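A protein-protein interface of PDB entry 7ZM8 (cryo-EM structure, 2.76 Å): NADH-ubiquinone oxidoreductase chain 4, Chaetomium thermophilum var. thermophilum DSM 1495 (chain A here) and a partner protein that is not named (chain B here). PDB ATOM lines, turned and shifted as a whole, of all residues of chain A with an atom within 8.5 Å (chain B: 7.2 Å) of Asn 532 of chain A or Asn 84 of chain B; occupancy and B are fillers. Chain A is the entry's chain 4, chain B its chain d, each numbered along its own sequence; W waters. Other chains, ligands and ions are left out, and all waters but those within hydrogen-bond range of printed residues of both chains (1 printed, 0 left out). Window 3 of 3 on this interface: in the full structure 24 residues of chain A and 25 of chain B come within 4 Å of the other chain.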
ATOM      1  N   ILE A 529      23.566 -14.885  15.099  1.00  0.00           N
ATOM      2  CA  ILE A 529      22.226 -14.980  15.657  1.00  0.00           C
ATOM      3  C   ILE A 529      21.235 -14.434  14.646  1.00  0.00           C
ATOM      4  O   ILE A 529      21.592 -13.705  13.720  1.00  0.00           O
ATOM      5  CB  ILE A 529      22.070 -14.222  16.993  1.00  0.00           C
ATOM      6  CG1 ILE A 529      22.735 -12.852  16.916  1.00  0.00           C
ATOM      7  CG2 ILE A 529      22.617 -15.040  18.152  1.00  0.00           C
ATOM      8  CD1 ILE A 529      22.460 -12.003  18.110  1.00  0.00           C
ATOM      9  N   GLU A 530      19.979 -14.807  14.835  1.00  0.00           N
ATOM     10  CA  GLU A 530      18.833 -14.272  14.132  1.00  0.00           C
ATOM     11  C   GLU A 530      17.925 -13.551  15.116  1.00  0.00           C
ATOM     12  O   GLU A 530      17.752 -14.015  16.246  1.00  0.00           O
ATOM     13  CB  GLU A 530      18.056 -15.382  13.418  1.00  0.00           C
ATOM     14  CG  GLU A 530      18.782 -15.946  12.210  1.00  0.00           C
ATOM     15  CD  GLU A 530      18.919 -14.926  11.094  1.00  0.00           C
ATOM     16  OE1 GLU A 530      17.922 -14.229  10.804  1.00  0.00           O
ATOM     17  OE2 GLU A 530      20.025 -14.805  10.521  1.00  0.00           O
ATOM     18  N   PRO A 531      17.345 -12.414  14.728  1.00  0.00           N
ATOM     19  CA  PRO A 531      16.724 -11.526  15.725  1.00  0.00           C
ATOM     20  C   PRO A 531      15.531 -12.112  16.447  1.00  0.00           C
ATOM     21  O   PRO A 531      15.202 -11.635  17.538  1.00  0.00           O
ATOM     22  CB  PRO A 531      16.321 -10.301  14.898  1.00  0.00           C
ATOM     23  CG  PRO A 531      16.247 -10.786  13.517  1.00  0.00           C
ATOM     24  CD  PRO A 531      17.261 -11.863  13.371  1.00  0.00           C
ATOM     25  N   ASN A 532      14.895 -13.149  15.914  1.00  0.00           N
ATOM     26  CA  ASN A 532      13.652 -13.645  16.551  1.00  0.00           C
ATOM     27  C   ASN A 532      13.855 -15.087  16.988  1.00  0.00           C
ATOM     28  O   ASN A 532      12.954 -15.647  17.624  1.00  0.00           O
ATOM     29  CB  ASN A 532      12.465 -13.476  15.606  1.00  0.00           C
ATOM     30  CG  ASN A 532      12.193 -12.026  15.271  1.00  0.00           C
ATOM     31  OD1 ASN A 532      12.453 -11.576  14.158  1.00  0.00           O
ATOM     32  ND2 ASN A 532      11.688 -11.278  16.238  1.00  0.00           N
ATOM     33  N   ALA A 533      15.007 -15.659  16.651  1.00  0.00           N
ATOM     34  CA  ALA A 533      15.273 -17.075  16.979  1.00  0.00           C
ATOM     35  C   ALA A 533      16.242 -17.172  18.144  1.00  0.00           C
ATOM     36  O   ALA A 533      16.552 -18.288  18.560  1.00  0.00           O
ATOM     37  CB  ALA A 533      15.876 -17.735  15.771  1.00  0.00           C
ATOM     38  N   SER A 534      16.719 -16.042  18.638  1.00  0.00           N
ATOM     39  CA  SER A 534      17.772 -16.139  19.669  1.00  0.00           C
ATOM     40  C   SER A 534      17.302 -15.709  21.040  1.00  0.00           C
ATOM     41  O   SER A 534      16.188 -15.168  21.146  1.00  0.00           O
ATOM     42  CB  SER A 534      18.928 -15.278  19.279  1.00  0.00           C
ATOM     43  OG  SER A 534      18.492 -13.994  18.862  1.00  0.00           O
ATOM     44  N   TYR A 535      18.143 -15.943  22.035  1.00  0.00           N
ATOM     45  CA  TYR A 535      17.874 -15.454  23.385  1.00  0.00           C
ATOM     46  C   TYR A 535      16.427 -15.729  23.790  1.00  0.00           C
ATOM     47  O   TYR A 535      15.628 -14.824  24.035  1.00  0.00           O
ATOM     48  CB  TYR A 535      18.224 -13.971  23.490  1.00  0.00           C
ATOM     49  CG  TYR A 535      19.701 -13.732  23.331  1.00  0.00           C
ATOM     50  CD1 TYR A 535      20.586 -14.102  24.321  1.00  0.00           C
ATOM     51  CD2 TYR A 535      20.210 -13.163  22.179  1.00  0.00           C
ATOM     52  CE1 TYR A 535      21.932 -13.906  24.176  1.00  0.00           C
ATOM     53  CE2 TYR A 535      21.556 -12.964  22.028  1.00  0.00           C
ATOM     54  CZ  TYR A 535      22.412 -13.337  23.033  1.00  0.00           C
ATOM     55  OH  TYR A 535      23.760 -13.143  22.900  1.00  0.00           O
ATOM     56  N   LEU A 536      16.108 -17.015  23.850  1.00  0.00           N
ATOM     57  CA  LEU A 536      14.755 -17.461  24.123  1.00  0.00           C
ATOM     58  C   LEU A 536      14.491 -17.520  25.622  1.00  0.00           C
ATOM     59  O   LEU A 536      15.385 -17.803  26.422  1.00  0.00           O
ATOM     60  CB  LEU A 536      14.519 -18.835  23.504  1.00  0.00           C
ATOM     61  CG  LEU A 536      14.726 -18.914  21.998  1.00  0.00           C
ATOM     62  CD1 LEU A 536      14.378 -20.298  21.495  1.00  0.00           C
ATOM     63  CD2 LEU A 536      13.876 -17.866  21.319  1.00  0.00           C
ATOM     64  N   GLN B  45      12.854 -25.699  13.481  1.00  0.00           N
ATOM     65  CA  GLN B  45      12.336 -24.527  12.767  1.00  0.00           C
ATOM     66  C   GLN B  45      12.575 -24.661  11.266  1.00  0.00           C
ATOM     67  O   GLN B  45      11.711 -24.233  10.499  1.00  0.00           O
ATOM     68  CB  GLN B  45      12.926 -23.282  13.422  1.00  0.00           C
ATOM     69  CG  GLN B  45      12.277 -22.924  14.744  1.00  0.00           C
ATOM     70  CD  GLN B  45      10.776 -22.865  14.622  1.00  0.00           C
ATOM     71  OE1 GLN B  45      10.054 -23.572  15.314  1.00  0.00           O
ATOM     72  NE2 GLN B  45      10.294 -22.025  13.724  1.00  0.00           N
ATOM     73  N   VAL B  46      13.723 -25.191  10.863  1.00  0.00           N
ATOM     74  CA  VAL B  46      14.053 -25.268   9.416  1.00  0.00           C
ATOM     75  C   VAL B  46      13.326 -26.465   8.803  1.00  0.00           C
ATOM     76  O   VAL B  46      12.951 -26.381   7.624  1.00  0.00           O
ATOM     77  CB  VAL B  46      15.573 -25.241   9.154  1.00  0.00           C
ATOM     78  CG1 VAL B  46      15.910 -25.430   7.685  1.00  0.00           C
ATOM     79  CG2 VAL B  46      16.217 -23.973   9.688  1.00  0.00           C
ATOM     80  N   ARG B  77       3.204 -18.670   5.427  1.00  0.00           N
ATOM     81  CA  ARG B  77       3.942 -19.405   6.445  1.00  0.00           C
ATOM     82  C   ARG B  77       5.371 -19.677   6.001  1.00  0.00           C
ATOM     83  O   ARG B  77       6.308 -19.562   6.795  1.00  0.00           O
ATOM     84  CB  ARG B  77       3.219 -20.710   6.768  1.00  0.00           C
ATOM     85  CG  ARG B  77       3.732 -21.411   8.002  1.00  0.00           C
ATOM     86  CD  ARG B  77       3.488 -20.578   9.232  1.00  0.00           C
ATOM     87  NE  ARG B  77       4.246 -21.075  10.373  1.00  0.00           N
ATOM     88  CZ  ARG B  77       5.174 -20.373  11.009  1.00  0.00           C
ATOM     89  NH1 ARG B  77       5.820 -20.905  12.035  1.00  0.00           N
ATOM     90  NH2 ARG B  77       5.457 -19.141  10.616  1.00  0.00           N
ATOM     91  N   TYR B  78       5.558 -20.039   4.731  1.00  0.00           N
ATOM     92  CA  TYR B  78       6.900 -20.321   4.240  1.00  0.00           C
ATOM     93  C   TYR B  78       7.760 -19.065   4.216  1.00  0.00           C
ATOM     94  O   TYR B  78       8.961 -19.122   4.499  1.00  0.00           O
ATOM     95  CB  TYR B  78       6.839 -20.951   2.852  1.00  0.00           C
ATOM     96  CG  TYR B  78       8.208 -21.194   2.281  1.00  0.00           C
ATOM     97  CD1 TYR B  78       9.017 -22.207   2.776  1.00  0.00           C
ATOM     98  CD2 TYR B  78       8.712 -20.385   1.279  1.00  0.00           C
ATOM     99  CE1 TYR B  78      10.278 -22.416   2.274  1.00  0.00           C
ATOM    100  CE2 TYR B  78       9.970 -20.586   0.776  1.00  0.00           C
ATOM    101  CZ  TYR B  78      10.749 -21.603   1.274  1.00  0.00           C
ATOM    102  OH  TYR B  78      12.003 -21.808   0.762  1.00  0.00           O
ATOM    103  N   LEU B  79       7.169 -17.925   3.873  1.00  0.00           N
ATOM    104  CA  LEU B  79       7.943 -16.693   3.831  1.00  0.00           C
ATOM    105  C   LEU B  79       8.245 -16.175   5.225  1.00  0.00           C
ATOM    106  O   LEU B  79       9.272 -15.520   5.430  1.00  0.00           O
ATOM    107  CB  LEU B  79       7.202 -15.637   3.025  1.00  0.00           C
ATOM    108  CG  LEU B  79       7.189 -15.819   1.519  1.00  0.00           C
ATOM    109  CD1 LEU B  79       6.329 -14.744   0.920  1.00  0.00           C
ATOM    110  CD2 LEU B  79       8.590 -15.742   0.979  1.00  0.00           C
ATOM    111  N   GLN B  80       7.356 -16.430   6.182  1.00  0.00           N
ATOM    112  CA  GLN B  80       7.663 -16.142   7.578  1.00  0.00           C
ATOM    113  C   GLN B  80       8.845 -16.971   8.055  1.00  0.00           C
ATOM    114  O   GLN B  80       9.823 -16.433   8.582  1.00  0.00           O
ATOM    115  CB  GLN B  80       6.433 -16.407   8.438  1.00  0.00           C
ATOM    116  CG  GLN B  80       5.291 -15.457   8.161  1.00  0.00           C
ATOM    117  CD  GLN B  80       4.069 -15.748   8.998  1.00  0.00           C
ATOM    118  OE1 GLN B  80       4.037 -16.715   9.756  1.00  0.00           O
ATOM    119  NE2 GLN B  80       3.047 -14.917   8.859  1.00  0.00           N
ATOM    120  N   LEU B  81       8.781 -18.287   7.853  1.00  0.00           N
ATOM    121  CA  LEU B  81       9.857 -19.159   8.304  1.00  0.00           C
ATOM    122  C   LEU B  81      11.167 -18.861   7.592  1.00  0.00           C
ATOM    123  O   LEU B  81      12.233 -18.947   8.205  1.00  0.00           O
ATOM    124  CB  LEU B  81       9.467 -20.621   8.100  1.00  0.00           C
ATOM    125  CG  LEU B  81       8.315 -21.155   8.950  1.00  0.00           C
ATOM    126  CD1 LEU B  81       7.564 -22.223   8.191  1.00  0.00           C
ATOM    127  CD2 LEU B  81       8.820 -21.707  10.265  1.00  0.00           C
ATOM    128  N   LEU B  82      11.109 -18.517   6.307  1.00  0.00           N
ATOM    129  CA  LEU B  82      12.326 -18.274   5.542  1.00  0.00           C
ATOM    130  C   LEU B  82      13.115 -17.092   6.087  1.00  0.00           C
ATOM    131  O   LEU B  82      14.348 -17.080   6.012  1.00  0.00           O
ATOM    132  CB  LEU B  82      11.977 -18.043   4.076  1.00  0.00           C
ATOM    133  CG  LEU B  82      13.142 -18.027   3.091  1.00  0.00           C
ATOM    134  CD1 LEU B  82      13.936 -19.315   3.173  1.00  0.00           C
ATOM    135  CD2 LEU B  82      12.618 -17.793   1.698  1.00  0.00           C
ATOM    136  N   ALA B  83      12.431 -16.090   6.624  1.00  0.00           N
ATOM    137  CA  ALA B  83      13.101 -14.933   7.189  1.00  0.00           C
ATOM    138  C   ALA B  83      13.566 -15.149   8.620  1.00  0.00           C
ATOM    139  O   ALA B  83      14.348 -14.340   9.125  1.00  0.00           O
ATOM    140  CB  ALA B  83      12.174 -13.722   7.137  1.00  0.00           C
ATOM    141  N   ASN B  84      13.123 -16.214   9.278  1.00  0.00           N
ATOM    142  CA  ASN B  84      13.344 -16.386  10.703  1.00  0.00           C
ATOM    143  C   ASN B  84      14.107 -17.643  11.079  1.00  0.00           C
ATOM    144  O   ASN B  84      14.714 -17.672  12.149  1.00  0.00           O
ATOM    145  CB  ASN B  84      12.002 -16.389  11.445  1.00  0.00           C
ATOM    146  CG  ASN B  84      11.312 -15.046  11.400  1.00  0.00           C
ATOM    147  OD1 ASN B  84      11.188 -14.362  12.412  1.00  0.00           O
ATOM    148  ND2 ASN B  84      10.858 -14.657  10.217  1.00  0.00           N
ATOM    149  N   ALA B  85      14.139 -18.639  10.212  1.00  0.00           N
ATOM    150  CA  ALA B  85      14.844 -19.836  10.682  1.00  0.00           C
ATOM    151  C   ALA B  85      16.088 -20.073   9.855  1.00  0.00           C
ATOM    152  O   ALA B  85      15.964 -20.227   8.665  1.00  0.00           O
ATOM    153  CB  ALA B  85      13.927 -21.013  10.594  1.00  0.00           C
ATOM    154  N   LYS B  86      17.242 -20.017  10.499  1.00  0.00           N
ATOM    155  CA  LYS B  86      18.509 -20.381   9.856  1.00  0.00           C
ATOM    156  C   LYS B  86      19.186 -21.209  10.933  1.00  0.00           C
ATOM    157  O   LYS B  86      18.742 -21.108  12.073  1.00  0.00           O
ATOM    158  CB  LYS B  86      19.337 -19.155   9.488  1.00  0.00           C
ATOM    159  CG  LYS B  86      18.963 -18.448   8.198  1.00  0.00           C
ATOM    160  CD  LYS B  86      20.147 -17.807   7.527  1.00  0.00           C
ATOM    161  CE  LYS B  86      21.050 -18.831   6.882  1.00  0.00           C
ATOM    162  NZ  LYS B  86      20.344 -19.596   5.829  1.00  0.00           N
ATOM    163  N   VAL B  87      20.125 -22.067  10.582  1.00  0.00           N
ATOM    164  CA  VAL B  87      20.862 -22.759  11.668  1.00  0.00           C
ATOM    165  C   VAL B  87      22.087 -21.885  11.907  1.00  0.00           C
ATOM    166  O   VAL B  87      22.958 -21.836  11.034  1.00  0.00           O
ATOM    167  CB  VAL B  87      21.137 -24.247  11.365  1.00  0.00           C
ATOM    168  CG1 VAL B  87      22.141 -24.834  12.338  1.00  0.00           C
ATOM    169  CG2 VAL B  87      19.860 -25.070  11.345  1.00  0.00           C
ATOM    170  N   LYS B  88      22.092 -21.146  13.013  1.00  0.00           N
ATOM    171  CA  LYS B  88      23.167 -20.152  13.245  1.00  0.00           C
ATOM    172  C   LYS B  88      24.139 -20.649  14.301  1.00  0.00           C
ATOM    173  O   LYS B  88      25.171 -20.023  14.455  1.00  0.00           O
ATOM    174  CB  LYS B  88      22.527 -18.803  13.571  1.00  0.00           C
ATOM    175  CG  LYS B  88      21.698 -18.186  12.455  1.00  0.00           C
ATOM    176  CD  LYS B  88      22.525 -17.777  11.263  1.00  0.00           C
ATOM    177  CE  LYS B  88      23.559 -16.730  11.610  1.00  0.00           C
ATOM    178  NZ  LYS B  88      24.531 -16.525  10.513  1.00  0.00           N
HETATM  179  O   HOH W   1      16.565 -16.343   9.037  1.00  0.00           O
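O of Glu 530 of chain A sits at hydrogen-bond distance from OG of Ser 534 of chain A.
O of Gln 80 of chain B is in hydrogen-bond range of ND2 of Asn 84 of chain B, at 2.6 Å.
Lys 88 of chain B touches Ile 529 of chain A (CE to N, 3.9 Å).
Ala 83 of chain B touches Glu 530 of chain A.
CG of Glu 530 of chain A touches CG of Lys 88 of chain B, 3.7 Å away.
Asn 532 of chain A touches Asn 84 of chain B (OD1 to OD1, 3.5 Å).
Ala 533 of chain A touches Asn 84 of chain B (CB to O, 3.8 Å).
Of the printed residues of chain B, Ile 529 of chain A touches Lys 88.
Asn 532 of chain A touches just one residue of chain B: Asn 84 (3.5 Å).
Of the printed residues of chain B, Ala 533 of chain A touches Asn 84 (3.8 Å).
Gln 80 of chain B touches none of the printed residues of chain A.
Ala 83 of chain B touches one residue of chain A.
Of chain A, only Asn 532 and Ala 533 come within 4 Å of Asn 84 of chain B.
The nearest residue of chain B that does not touch Asn 532 of chain A is Ala 83 of chain B (6.0 Å).
The nearest printed residue of chain B that does not touch Ala 533 of chain A is Ala 85 of chain B (5.6 Å).
Printed residues of chain A that touch a printed residue of chain B: Ile 529, Glu 530, Asn 532 and Ala 533.
Of the 14 printed residues of chain B, 3 touch a printed residue of chain A.
Printed residues of chain B that touch a printed residue of chain A: Ala 83, Asn 84 and Lys 88.
Along chain B the printed residues that touch a printed residue of chain A span positions 83 to 88.
Among the printed residues, 5 pairs touch across the chains.
Water W1 lies within hydrogen-bond range of O of Ala 83 of chain B, OE1 of Glu 530 of chain A and N of Asn 84 of chain B.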
